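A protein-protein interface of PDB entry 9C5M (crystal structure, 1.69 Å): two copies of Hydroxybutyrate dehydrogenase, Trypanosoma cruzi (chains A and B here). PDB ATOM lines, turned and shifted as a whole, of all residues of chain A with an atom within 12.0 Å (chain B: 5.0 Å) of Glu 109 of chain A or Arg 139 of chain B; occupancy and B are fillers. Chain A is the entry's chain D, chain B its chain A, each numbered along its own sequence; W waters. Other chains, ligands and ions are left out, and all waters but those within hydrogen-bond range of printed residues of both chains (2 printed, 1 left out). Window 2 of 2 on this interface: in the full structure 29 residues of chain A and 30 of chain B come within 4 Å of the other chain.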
ATOM      1  N   HIS A 104      32.491   0.574  -3.504  1.00  0.00           N
ATOM      2  CA  HIS A 104      31.134   1.060  -3.279  1.00  0.00           C
ATOM      3  C   HIS A 104      30.751   1.959  -4.446  1.00  0.00           C
ATOM      4  O   HIS A 104      31.445   2.942  -4.723  1.00  0.00           O
ATOM      5  CB  HIS A 104      31.009   1.823  -1.969  1.00  0.00           C
ATOM      6  CG  HIS A 104      29.622   2.311  -1.707  1.00  0.00           C
ATOM      7  ND1 HIS A 104      28.651   1.515  -1.137  1.00  0.00           N
ATOM      8  CD2 HIS A 104      29.026   3.496  -1.978  1.00  0.00           C
ATOM      9  CE1 HIS A 104      27.524   2.199  -1.045  1.00  0.00           C
ATOM     10  NE2 HIS A 104      27.725   3.404  -1.545  1.00  0.00           N
ATOM     11  N   VAL A 105      29.649   1.640  -5.116  1.00  0.00           N
ATOM     12  CA  VAL A 105      29.214   2.354  -6.313  1.00  0.00           C
ATOM     13  C   VAL A 105      28.132   3.354  -5.918  1.00  0.00           C
ATOM     14  O   VAL A 105      27.102   2.977  -5.343  1.00  0.00           O
ATOM     15  CB  VAL A 105      28.713   1.368  -7.382  1.00  0.00           C
ATOM     16  CG1 VAL A 105      28.309   2.083  -8.667  1.00  0.00           C
ATOM     17  CG2 VAL A 105      29.796   0.325  -7.658  1.00  0.00           C
ATOM     18  N   SER A 106      28.369   4.634  -6.229  1.00  0.00           N
ATOM     19  CA  SER A 106      27.441   5.717  -5.934  1.00  0.00           C
ATOM     20  C   SER A 106      27.808   6.977  -6.706  1.00  0.00           C
ATOM     21  O   SER A 106      28.998   7.265  -6.879  1.00  0.00           O
ATOM     22  CB  SER A 106      27.434   6.039  -4.437  1.00  0.00           C
ATOM     23  OG  SER A 106      26.668   7.205  -4.171  1.00  0.00           O
ATOM     24  N   PRO A 107      26.832   7.766  -7.165  1.00  0.00           N
ATOM     25  CA  PRO A 107      27.158   9.107  -7.667  1.00  0.00           C
ATOM     26  C   PRO A 107      27.832   9.922  -6.576  1.00  0.00           C
ATOM     27  O   PRO A 107      27.627   9.685  -5.382  1.00  0.00           O
ATOM     28  CB  PRO A 107      25.797   9.707  -8.041  1.00  0.00           C
ATOM     29  CG  PRO A 107      24.875   8.569  -8.166  1.00  0.00           C
ATOM     30  CD  PRO A 107      25.396   7.451  -7.292  1.00  0.00           C
ATOM     31  N   VAL A 108      28.623  10.911  -6.993  1.00  0.00           N
ATOM     32  CA  VAL A 108      29.387  11.695  -6.029  1.00  0.00           C
ATOM     33  C   VAL A 108      28.460  12.369  -5.024  1.00  0.00           C
ATOM     34  O   VAL A 108      28.747  12.407  -3.821  1.00  0.00           O
ATOM     35  CB  VAL A 108      30.265  12.731  -6.751  1.00  0.00           C
ATOM     36  CG1 VAL A 108      30.920  13.658  -5.730  1.00  0.00           C
ATOM     37  CG2 VAL A 108      31.313  12.044  -7.585  1.00  0.00           C
ATOM     38  N   GLU A 109      27.327  12.907  -5.499  1.00  0.00           N
ATOM     39  CA  GLU A 109      26.480  13.748  -4.653  1.00  0.00           C
ATOM     40  C   GLU A 109      25.965  13.003  -3.430  1.00  0.00           C
ATOM     41  O   GLU A 109      25.791  13.596  -2.359  1.00  0.00           O
ATOM     42  CB  GLU A 109      25.288  14.283  -5.448  1.00  0.00           C
ATOM     43  CG  GLU A 109      25.631  15.284  -6.509  1.00  0.00           C
ATOM     44  CD  GLU A 109      25.921  14.650  -7.853  1.00  0.00           C
ATOM     45  OE1 GLU A 109      26.111  13.415  -7.919  1.00  0.00           O
ATOM     46  OE2 GLU A 109      25.961  15.403  -8.847  1.00  0.00           O
ATOM     47  N   THR A 110      25.675  11.717  -3.581  1.00  0.00           N
ATOM     48  CA  THR A 110      25.103  10.912  -2.513  1.00  0.00           C
ATOM     49  C   THR A 110      26.098   9.909  -1.952  1.00  0.00           C
ATOM     50  O   THR A 110      25.697   9.001  -1.220  1.00  0.00           O
ATOM     51  CB  THR A 110      23.849  10.193  -3.018  1.00  0.00           C
ATOM     52  OG1 THR A 110      24.147   9.484  -4.229  1.00  0.00           O
ATOM     53  CG2 THR A 110      22.734  11.188  -3.284  1.00  0.00           C
ATOM     54  N   PHE A 111      27.377  10.046  -2.275  1.00  0.00           N
ATOM     55  CA  PHE A 111      28.365   9.069  -1.825  1.00  0.00           C
ATOM     56  C   PHE A 111      28.458   9.159  -0.306  1.00  0.00           C
ATOM     57  O   PHE A 111      28.751  10.239   0.216  1.00  0.00           O
ATOM     58  CB  PHE A 111      29.724   9.337  -2.482  1.00  0.00           C
ATOM     59  CG  PHE A 111      30.570   8.106  -2.633  1.00  0.00           C
ATOM     60  CD1 PHE A 111      31.185   7.531  -1.529  1.00  0.00           C
ATOM     61  CD2 PHE A 111      30.740   7.518  -3.878  1.00  0.00           C
ATOM     62  CE1 PHE A 111      31.950   6.390  -1.659  1.00  0.00           C
ATOM     63  CE2 PHE A 111      31.507   6.374  -4.023  1.00  0.00           C
ATOM     64  CZ  PHE A 111      32.117   5.805  -2.906  1.00  0.00           C
ATOM     65  N   PRO A 112      28.204   8.083   0.443  1.00  0.00           N
ATOM     66  CA  PRO A 112      28.250   8.204   1.909  1.00  0.00           C
ATOM     67  C   PRO A 112      29.643   8.561   2.413  1.00  0.00           C
ATOM     68  O   PRO A 112      30.648   7.995   1.980  1.00  0.00           O
ATOM     69  CB  PRO A 112      27.810   6.818   2.399  1.00  0.00           C
ATOM     70  CG  PRO A 112      27.066   6.225   1.268  1.00  0.00           C
ATOM     71  CD  PRO A 112      27.735   6.750   0.023  1.00  0.00           C
ATOM     72  N   SER A 113      29.691   9.490   3.371  1.00  0.00           N
ATOM     73  CA  SER A 113      30.977   9.942   3.896  1.00  0.00           C
ATOM     74  C   SER A 113      31.762   8.788   4.509  1.00  0.00           C
ATOM     75  O   SER A 113      32.979   8.665   4.298  1.00  0.00           O
ATOM     76  CB  SER A 113      30.766  11.044   4.932  1.00  0.00           C
ATOM     77  OG  SER A 113      31.986  11.364   5.582  1.00  0.00           O
ATOM     78  N   ASP A 114      31.082   7.934   5.281  1.00  0.00           N
ATOM     79  CA  ASP A 114      31.761   6.806   5.911  1.00  0.00           C
ATOM     80  C   ASP A 114      32.323   5.839   4.870  1.00  0.00           C
ATOM     81  O   ASP A 114      33.403   5.266   5.066  1.00  0.00           O
ATOM     82  CB  ASP A 114      30.805   6.074   6.860  1.00  0.00           C
ATOM     83  CG  ASP A 114      30.567   6.827   8.172  1.00  0.00           C
ATOM     84  OD1 ASP A 114      31.180   7.895   8.395  1.00  0.00           O
ATOM     85  OD2 ASP A 114      29.758   6.331   8.989  1.00  0.00           O
ATOM     86  N   LYS A 115      31.605   5.630   3.759  1.00  0.00           N
ATOM     87  CA  LYS A 115      32.110   4.735   2.717  1.00  0.00           C
ATOM     88  C   LYS A 115      33.321   5.338   2.006  1.00  0.00           C
ATOM     89  O   LYS A 115      34.271   4.618   1.673  1.00  0.00           O
ATOM     90  CB  LYS A 115      31.021   4.413   1.692  1.00  0.00           C
ATOM     91  CG  LYS A 115      29.778   3.762   2.278  1.00  0.00           C
ATOM     92  CD  LYS A 115      29.773   2.238   2.131  1.00  0.00           C
ATOM     93  CE  LYS A 115      31.063   1.594   2.618  1.00  0.00           C
ATOM     94  NZ  LYS A 115      30.911   0.116   2.843  1.00  0.00           N
ATOM     95  N   TRP A 116      33.302   6.654   1.748  1.00  0.00           N
ATOM     96  CA  TRP A 116      34.496   7.310   1.220  1.00  0.00           C
ATOM     97  C   TRP A 116      35.685   7.049   2.138  1.00  0.00           C
ATOM     98  O   TRP A 116      36.750   6.591   1.694  1.00  0.00           O
ATOM     99  CB  TRP A 116      34.266   8.825   1.059  1.00  0.00           C
ATOM    100  CG  TRP A 116      35.521   9.565   0.626  1.00  0.00           C
ATOM    101  CD1 TRP A 116      36.581   9.923   1.415  1.00  0.00           C
ATOM    102  CD2 TRP A 116      35.842  10.016  -0.698  1.00  0.00           C
ATOM    103  NE1 TRP A 116      37.541  10.561   0.663  1.00  0.00           N
ATOM    104  CE2 TRP A 116      37.109  10.636  -0.635  1.00  0.00           C
ATOM    105  CE3 TRP A 116      35.173   9.965  -1.929  1.00  0.00           C
ATOM    106  CZ2 TRP A 116      37.725  11.184  -1.756  1.00  0.00           C
ATOM    107  CZ3 TRP A 116      35.780  10.510  -3.036  1.00  0.00           C
ATOM    108  CH2 TRP A 116      37.045  11.118  -2.944  1.00  0.00           C
ATOM    109  N   SER A 158      36.018   6.243 -13.821  1.00  0.00           N
ATOM    110  CA  SER A 158      34.744   5.633 -14.185  1.00  0.00           C
ATOM    111  C   SER A 158      33.634   6.251 -13.346  1.00  0.00           C
ATOM    112  O   SER A 158      33.832   6.529 -12.159  1.00  0.00           O
ATOM    113  CB  SER A 158      34.734   4.118 -13.959  1.00  0.00           C
ATOM    114  OG  SER A 158      35.709   3.483 -14.756  1.00  0.00           O
ATOM    115  N   MET A 159      32.458   6.420 -13.952  1.00  0.00           N
ATOM    116  CA  MET A 159      31.323   6.985 -13.237  1.00  0.00           C
ATOM    117  C   MET A 159      30.959   6.157 -12.009  1.00  0.00           C
ATOM    118  O   MET A 159      30.988   4.924 -12.028  1.00  0.00           O
ATOM    119  CB  MET A 159      30.105   7.082 -14.158  1.00  0.00           C
ATOM    120  CG  MET A 159      30.211   8.167 -15.206  1.00  0.00           C
ATOM    121  SD  MET A 159      28.698   8.338 -16.164  1.00  0.00           S
ATOM    122  CE  MET A 159      28.733   6.822 -17.112  1.00  0.00           C
ATOM    123  N   ASN A 160      30.602   6.871 -10.941  1.00  0.00           N
ATOM    124  CA  ASN A 160      30.049   6.329  -9.707  1.00  0.00           C
ATOM    125  C   ASN A 160      31.077   5.594  -8.872  1.00  0.00           C
ATOM    126  O   ASN A 160      30.712   4.852  -7.959  1.00  0.00           O
ATOM    127  CB  ASN A 160      28.847   5.438 -10.014  1.00  0.00           C
ATOM    128  CG  ASN A 160      27.791   6.177 -10.786  1.00  0.00           C
ATOM    129  OD1 ASN A 160      27.511   7.344 -10.503  1.00  0.00           O
ATOM    130  ND2 ASN A 160      27.244   5.537 -11.805  1.00  0.00           N
ATOM    131  N   LYS A 161      32.357   5.836  -9.119  1.00  0.00           N
ATOM    132  CA  LYS A 161      33.426   5.181  -8.376  1.00  0.00           C
ATOM    133  C   LYS A 161      34.451   6.204  -7.910  1.00  0.00           C
ATOM    134  O   LYS A 161      35.664   5.968  -7.939  1.00  0.00           O
ATOM    135  CB  LYS A 161      34.059   4.085  -9.225  1.00  0.00           C
ATOM    136  CG  LYS A 161      33.078   2.964  -9.555  1.00  0.00           C
ATOM    137  CD  LYS A 161      33.725   1.846 -10.353  1.00  0.00           C
ATOM    138  CE  LYS A 161      32.791   0.658 -10.431  1.00  0.00           C
ATOM    139  NZ  LYS A 161      33.361  -0.457 -11.245  1.00  0.00           N
ATOM    140  N   SER A 162      33.965   7.364  -7.458  1.00  0.00           N
ATOM    141  CA  SER A 162      34.866   8.466  -7.146  1.00  0.00           C
ATOM    142  C   SER A 162      35.867   8.083  -6.058  1.00  0.00           C
ATOM    143  O   SER A 162      37.072   8.327  -6.204  1.00  0.00           O
ATOM    144  CB  SER A 162      34.065   9.707  -6.741  1.00  0.00           C
ATOM    145  OG  SER A 162      33.246   9.475  -5.614  1.00  0.00           O
ATOM    146  N   ALA A 163      35.394   7.495  -4.953  1.00  0.00           N
ATOM    147  CA  ALA A 163      36.312   7.153  -3.871  1.00  0.00           C
ATOM    148  C   ALA A 163      37.328   6.116  -4.318  1.00  0.00           C
ATOM    149  O   ALA A 163      38.516   6.207  -3.993  1.00  0.00           O
ATOM    150  CB  ALA A 163      35.555   6.616  -2.658  1.00  0.00           C
ATOM    151  N   GLN B 132      30.795  17.675  -3.343  1.00  0.00           N
ATOM    152  CA  GLN B 132      29.509  17.065  -3.036  1.00  0.00           C
ATOM    153  C   GLN B 132      28.503  18.109  -2.592  1.00  0.00           C
ATOM    154  O   GLN B 132      27.331  18.069  -2.985  1.00  0.00           O
ATOM    155  CB  GLN B 132      29.730  16.014  -1.954  1.00  0.00           C
ATOM    156  CG  GLN B 132      28.521  15.316  -1.468  1.00  0.00           C
ATOM    157  CD  GLN B 132      28.900  14.195  -0.541  1.00  0.00           C
ATOM    158  OE1 GLN B 132      29.344  14.424   0.582  1.00  0.00           O
ATOM    159  NE2 GLN B 132      28.772  12.964  -1.020  1.00  0.00           N
ATOM    160  N   LEU B 135      27.658  20.471  -5.968  1.00  0.00           N
ATOM    161  CA  LEU B 135      27.117  19.967  -7.227  1.00  0.00           C
ATOM    162  C   LEU B 135      25.603  20.108  -7.358  1.00  0.00           C
ATOM    163  O   LEU B 135      25.135  20.388  -8.477  1.00  0.00           O
ATOM    164  CB  LEU B 135      27.532  18.502  -7.421  1.00  0.00           C
ATOM    165  CG  LEU B 135      28.890  18.245  -8.079  1.00  0.00           C
ATOM    166  CD1 LEU B 135      29.234  16.758  -7.986  1.00  0.00           C
ATOM    167  CD2 LEU B 135      28.920  18.695  -9.524  1.00  0.00           C
ATOM    168  N   PRO B 136      24.788  19.871  -6.329  1.00  0.00           N
ATOM    169  CA  PRO B 136      23.331  19.949  -6.556  1.00  0.00           C
ATOM    170  C   PRO B 136      22.872  21.288  -7.125  1.00  0.00           C
ATOM    171  O   PRO B 136      22.056  21.320  -8.062  1.00  0.00           O
ATOM    172  CB  PRO B 136      22.749  19.678  -5.157  1.00  0.00           C
ATOM    173  CG  PRO B 136      23.784  18.799  -4.481  1.00  0.00           C
ATOM    174  CD  PRO B 136      25.124  19.312  -4.999  1.00  0.00           C
ATOM    175  N   SER B 137      23.402  22.398  -6.600  1.00  0.00           N
ATOM    176  CA  SER B 137      23.052  23.716  -7.117  1.00  0.00           C
ATOM    177  C   SER B 137      23.530  23.890  -8.552  1.00  0.00           C
ATOM    178  O   SER B 137      22.815  24.458  -9.388  1.00  0.00           O
ATOM    179  CB  SER B 137      23.650  24.801  -6.222  1.00  0.00           C
ATOM    180  OG  SER B 137      23.343  26.097  -6.709  1.00  0.00           O
ATOM    181  N   MET B 138      24.746  23.430  -8.850  1.00  0.00           N
ATOM    182  CA  MET B 138      25.266  23.554 -10.206  1.00  0.00           C
ATOM    183  C   MET B 138      24.391  22.797 -11.190  1.00  0.00           C
ATOM    184  O   MET B 138      24.087  23.302 -12.278  1.00  0.00           O
ATOM    185  CB  MET B 138      26.704  23.046 -10.263  1.00  0.00           C
ATOM    186  CG  MET B 138      27.716  23.994  -9.639  1.00  0.00           C
ATOM    187  SD  MET B 138      29.309  23.177  -9.451  1.00  0.00           S
ATOM    188  CE  MET B 138      30.256  24.520  -8.720  1.00  0.00           C
ATOM    189  N   ARG B 139      23.962  21.589 -10.817  1.00  0.00           N
ATOM    190  CA  ARG B 139      23.068  20.817 -11.673  1.00  0.00           C
ATOM    191  C   ARG B 139      21.723  21.517 -11.859  1.00  0.00           C
ATOM    192  O   ARG B 139      21.183  21.544 -12.973  1.00  0.00           O
ATOM    193  CB  ARG B 139      22.858  19.418 -11.090  1.00  0.00           C
ATOM    194  CG  ARG B 139      24.069  18.488 -11.168  1.00  0.00           C
ATOM    195  CD  ARG B 139      23.686  17.061 -10.746  1.00  0.00           C
ATOM    196  NE  ARG B 139      24.758  16.095 -10.954  1.00  0.00           N
ATOM    197  CZ  ARG B 139      25.047  15.540 -12.122  1.00  0.00           C
ATOM    198  NH1 ARG B 139      24.414  15.894 -13.228  1.00  0.00           N
ATOM    199  NH2 ARG B 139      25.984  14.597 -12.179  1.00  0.00           N
ATOM    200  N   GLN B 140      21.160  22.076 -10.779  1.00  0.00           N
ATOM    201  CA  GLN B 140      19.898  22.809 -10.891  1.00  0.00           C
ATOM    202  C   GLN B 140      20.028  24.000 -11.834  1.00  0.00           C
ATOM    203  O   GLN B 140      19.116  24.288 -12.620  1.00  0.00           O
ATOM    204  CB  GLN B 140      19.452  23.264  -9.499  1.00  0.00           C
ATOM    205  CG  GLN B 140      18.172  24.068  -9.460  1.00  0.00           C
ATOM    206  CD  GLN B 140      17.207  23.548  -8.414  1.00  0.00           C
ATOM    207  OE1 GLN B 140      16.296  22.782  -8.725  1.00  0.00           O
ATOM    208  NE2 GLN B 140      17.409  23.955  -7.163  1.00  0.00           N
ATOM    209  N   ARG B 141      21.155  24.709 -11.765  1.00  0.00           N
ATOM    210  CA  ARG B 141      21.352  25.870 -12.624  1.00  0.00           C
ATOM    211  C   ARG B 141      21.862  25.517 -14.012  1.00  0.00           C
ATOM    212  O   ARG B 141      21.769  26.359 -14.911  1.00  0.00           O
ATOM    213  CB  ARG B 141      22.302  26.847 -11.941  1.00  0.00           C
ATOM    214  CG  ARG B 141      21.573  27.688 -10.921  1.00  0.00           C
ATOM    215  CD  ARG B 141      22.512  28.310  -9.932  1.00  0.00           C
ATOM    216  NE  ARG B 141      21.819  29.255  -9.067  1.00  0.00           N
ATOM    217  CZ  ARG B 141      21.575  30.517  -9.388  1.00  0.00           C
ATOM    218  NH1 ARG B 141      21.943  31.017 -10.556  1.00  0.00           N
ATOM    219  NH2 ARG B 141      20.951  31.299  -8.512  1.00  0.00           N
ATOM    220  N   GLY B 142      22.364  24.298 -14.216  1.00  0.00           N
ATOM    221  CA  GLY B 142      22.866  23.898 -15.515  1.00  0.00           C
ATOM    222  C   GLY B 142      24.224  24.450 -15.874  1.00  0.00           C
ATOM    223  O   GLY B 142      24.557  24.541 -17.058  1.00  0.00           O
ATOM    224  N   GLU B 181      30.794  12.043 -14.547  1.00  0.00           N
ATOM    225  CA  GLU B 181      29.428  12.032 -14.029  1.00  0.00           C
ATOM    226  C   GLU B 181      28.642  13.266 -14.450  1.00  0.00           C
ATOM    227  O   GLU B 181      27.406  13.256 -14.367  1.00  0.00           O
ATOM    228  CB  GLU B 181      29.430  11.932 -12.498  1.00  0.00           C
ATOM    229  CG  GLU B 181      29.922  10.584 -11.980  1.00  0.00           C
ATOM    230  CD  GLU B 181      29.837  10.432 -10.471  1.00  0.00           C
ATOM    231  OE1 GLU B 181      29.133  11.239  -9.819  1.00  0.00           O
ATOM    232  OE2 GLU B 181      30.498   9.509  -9.942  1.00  0.00           O
ATOM    233  N   THR B 182      29.332  14.333 -14.873  1.00  0.00           N
ATOM    234  CA  THR B 182      28.703  15.572 -15.315  1.00  0.00           C
ATOM    235  C   THR B 182      28.893  15.844 -16.808  1.00  0.00           C
ATOM    236  O   THR B 182      28.549  16.932 -17.277  1.00  0.00           O
ATOM    237  CB  THR B 182      29.253  16.768 -14.516  1.00  0.00           C
ATOM    238  OG1 THR B 182      30.682  16.828 -14.646  1.00  0.00           O
ATOM    239  CG2 THR B 182      28.866  16.664 -13.030  1.00  0.00           C
ATOM    240  N   THR B 185      26.392  17.738 -19.038  1.00  0.00           N
ATOM    241  CA  THR B 185      25.848  18.953 -18.459  1.00  0.00           C
ATOM    242  C   THR B 185      26.778  20.126 -18.752  1.00  0.00           C
ATOM    243  O   THR B 185      27.869  19.970 -19.309  1.00  0.00           O
ATOM    244  CB  THR B 185      25.667  18.827 -16.942  1.00  0.00           C
ATOM    245  OG1 THR B 185      26.945  18.949 -16.297  1.00  0.00           O
ATOM    246  CG2 THR B 185      25.021  17.499 -16.562  1.00  0.00           C
ATOM    247  N   ILE B 187      28.377  21.555 -16.419  1.00  0.00           N
ATOM    248  CA  ILE B 187      29.349  21.509 -15.329  1.00  0.00           C
ATOM    249  C   ILE B 187      30.587  20.786 -15.840  1.00  0.00           C
ATOM    250  O   ILE B 187      30.474  19.678 -16.379  1.00  0.00           O
ATOM    251  CB  ILE B 187      28.779  20.763 -14.107  1.00  0.00           C
ATOM    252  CG1 ILE B 187      27.457  21.381 -13.649  1.00  0.00           C
ATOM    253  CG2 ILE B 187      29.797  20.718 -12.979  1.00  0.00           C
ATOM    254  CD1 ILE B 187      26.635  20.446 -12.782  1.00  0.00           C
HETATM  255  O   HOH W   1      31.167   8.662  -7.470  1.00  0.00           O
HETATM  256  O   HOH W   2      26.934  12.661 -10.326  1.00  0.00           O
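The backbone carbonyl oxygen of Glu 109 of chain A sits at hydrogen-bond distance from the side-chain amide nitrogen of Gln 132 of chain B (3.3 Å). The backbone carbonyl oxygen of Val 108 of chain A lies within hydrogen-bond range of the side-chain amide nitrogen of Gln 132 of chain B, 2.9 Å away. The side-chain carboxylate (OE2) of Glu 109 of chain A lies within salt-bridge range of the guanidinium group (NE) of Arg 139 of chain B (2.5 Å). OE1 of Glu 181 of chain B lies within hydrogen-bond range of N of Val 108 of chain A (2.9 Å). The side-chain carboxylate (OE2) of Glu 181 of chain B is in hydrogen-bond range of the backbone NH (N) of Asn 160 of chain A, at 2.8 Å. The backbone carbonyl oxygen (O) of Phe 111 of chain A lies within hydrogen-bond range of the side-chain amide nitrogen (NE2) of Gln 132 of chain B, 3.0 Å away.
The side-chain hydroxyl (OG) of Ser 106 of chain A lies close to the backbone NH (N) of Phe 111 of chain A. The backbone NH of Ser 106 of chain A lies within hydrogen-bond range of the backbone carbonyl oxygen of Asn 160 of chain A, at 2.9 Å. The guanidinium group (NH2) of Arg 139 of chain B sits at hydrogen-bond distance from the backbone carbonyl oxygen (O) of Glu 181 of chain B (2.9 Å).
Glu 181 of chain B touches Pro 107 of chain A. OE2 of Glu 109 of chain A touches CD1 of Leu 135 of chain B, at 3.6 Å. Met 159 of chain A touches Glu 181 of chain B.
Glu 109 of chain A touches three residues of chain B. Arg 139 of chain B touches just one residue of chain A: Glu 109. No residue of chain A comes within 4 Å of Ser 137 of chain B. No residue of chain A comes within 4 Å of Met 138 of chain B. No residue of chain A comes within 4 Å of Thr 182 of chain B. Printed residues of chain B within 4 Å of Val 108 of chain A: Gln 132 and Glu 181. Printed residues of chain B within 4 Å of Pro 107 of chain A: Glu 181 (3.6 Å). Of the printed residues of chain A, Glu 181 of chain B touches Pro 107, Val 108, Met 159 and Asn 160. Printed residues of chain B within 4 Å of Asn 160 of chain A: Glu 181 (2.8 Å). Thr 185 of chain B touches none of the printed residues of chain A. The nearest printed residue of chain A that does not touch Leu 135 of chain B is Val 108 of chain A (4.2 Å).
Of the 19 printed residues of chain A, 6 touch a printed residue of chain B. Hydrophobic or aromatic side chains of chain A that line the printed part of chain B: Val 108 and Met 159. Hydrophobic or aromatic side chains of chain B within 4 Å of the printed part of chain A: Leu 135.
No position is printed for both chains.
Water W1 lies within hydrogen-bond range of the backbone carbonyl oxygen (O) of Ser 106 of chain A (2.6 Å), the side-chain carboxylate (OE2) of Glu 181 of chain B (2.7 Å), the side-chain hydroxyl (OG) of Ser 162 of chain A (2.9 Å), the backbone NH (N) of Val 108 of chain A (3.4 Å) and the backbone NH (N) of Lys 161 of chain A (3.5 Å). Water W2 lies within hydrogen-bond range of OE1 of Glu 109 of chain A, OE1 of Glu 181 of chain B and NH2 of Arg 139 of chain B.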
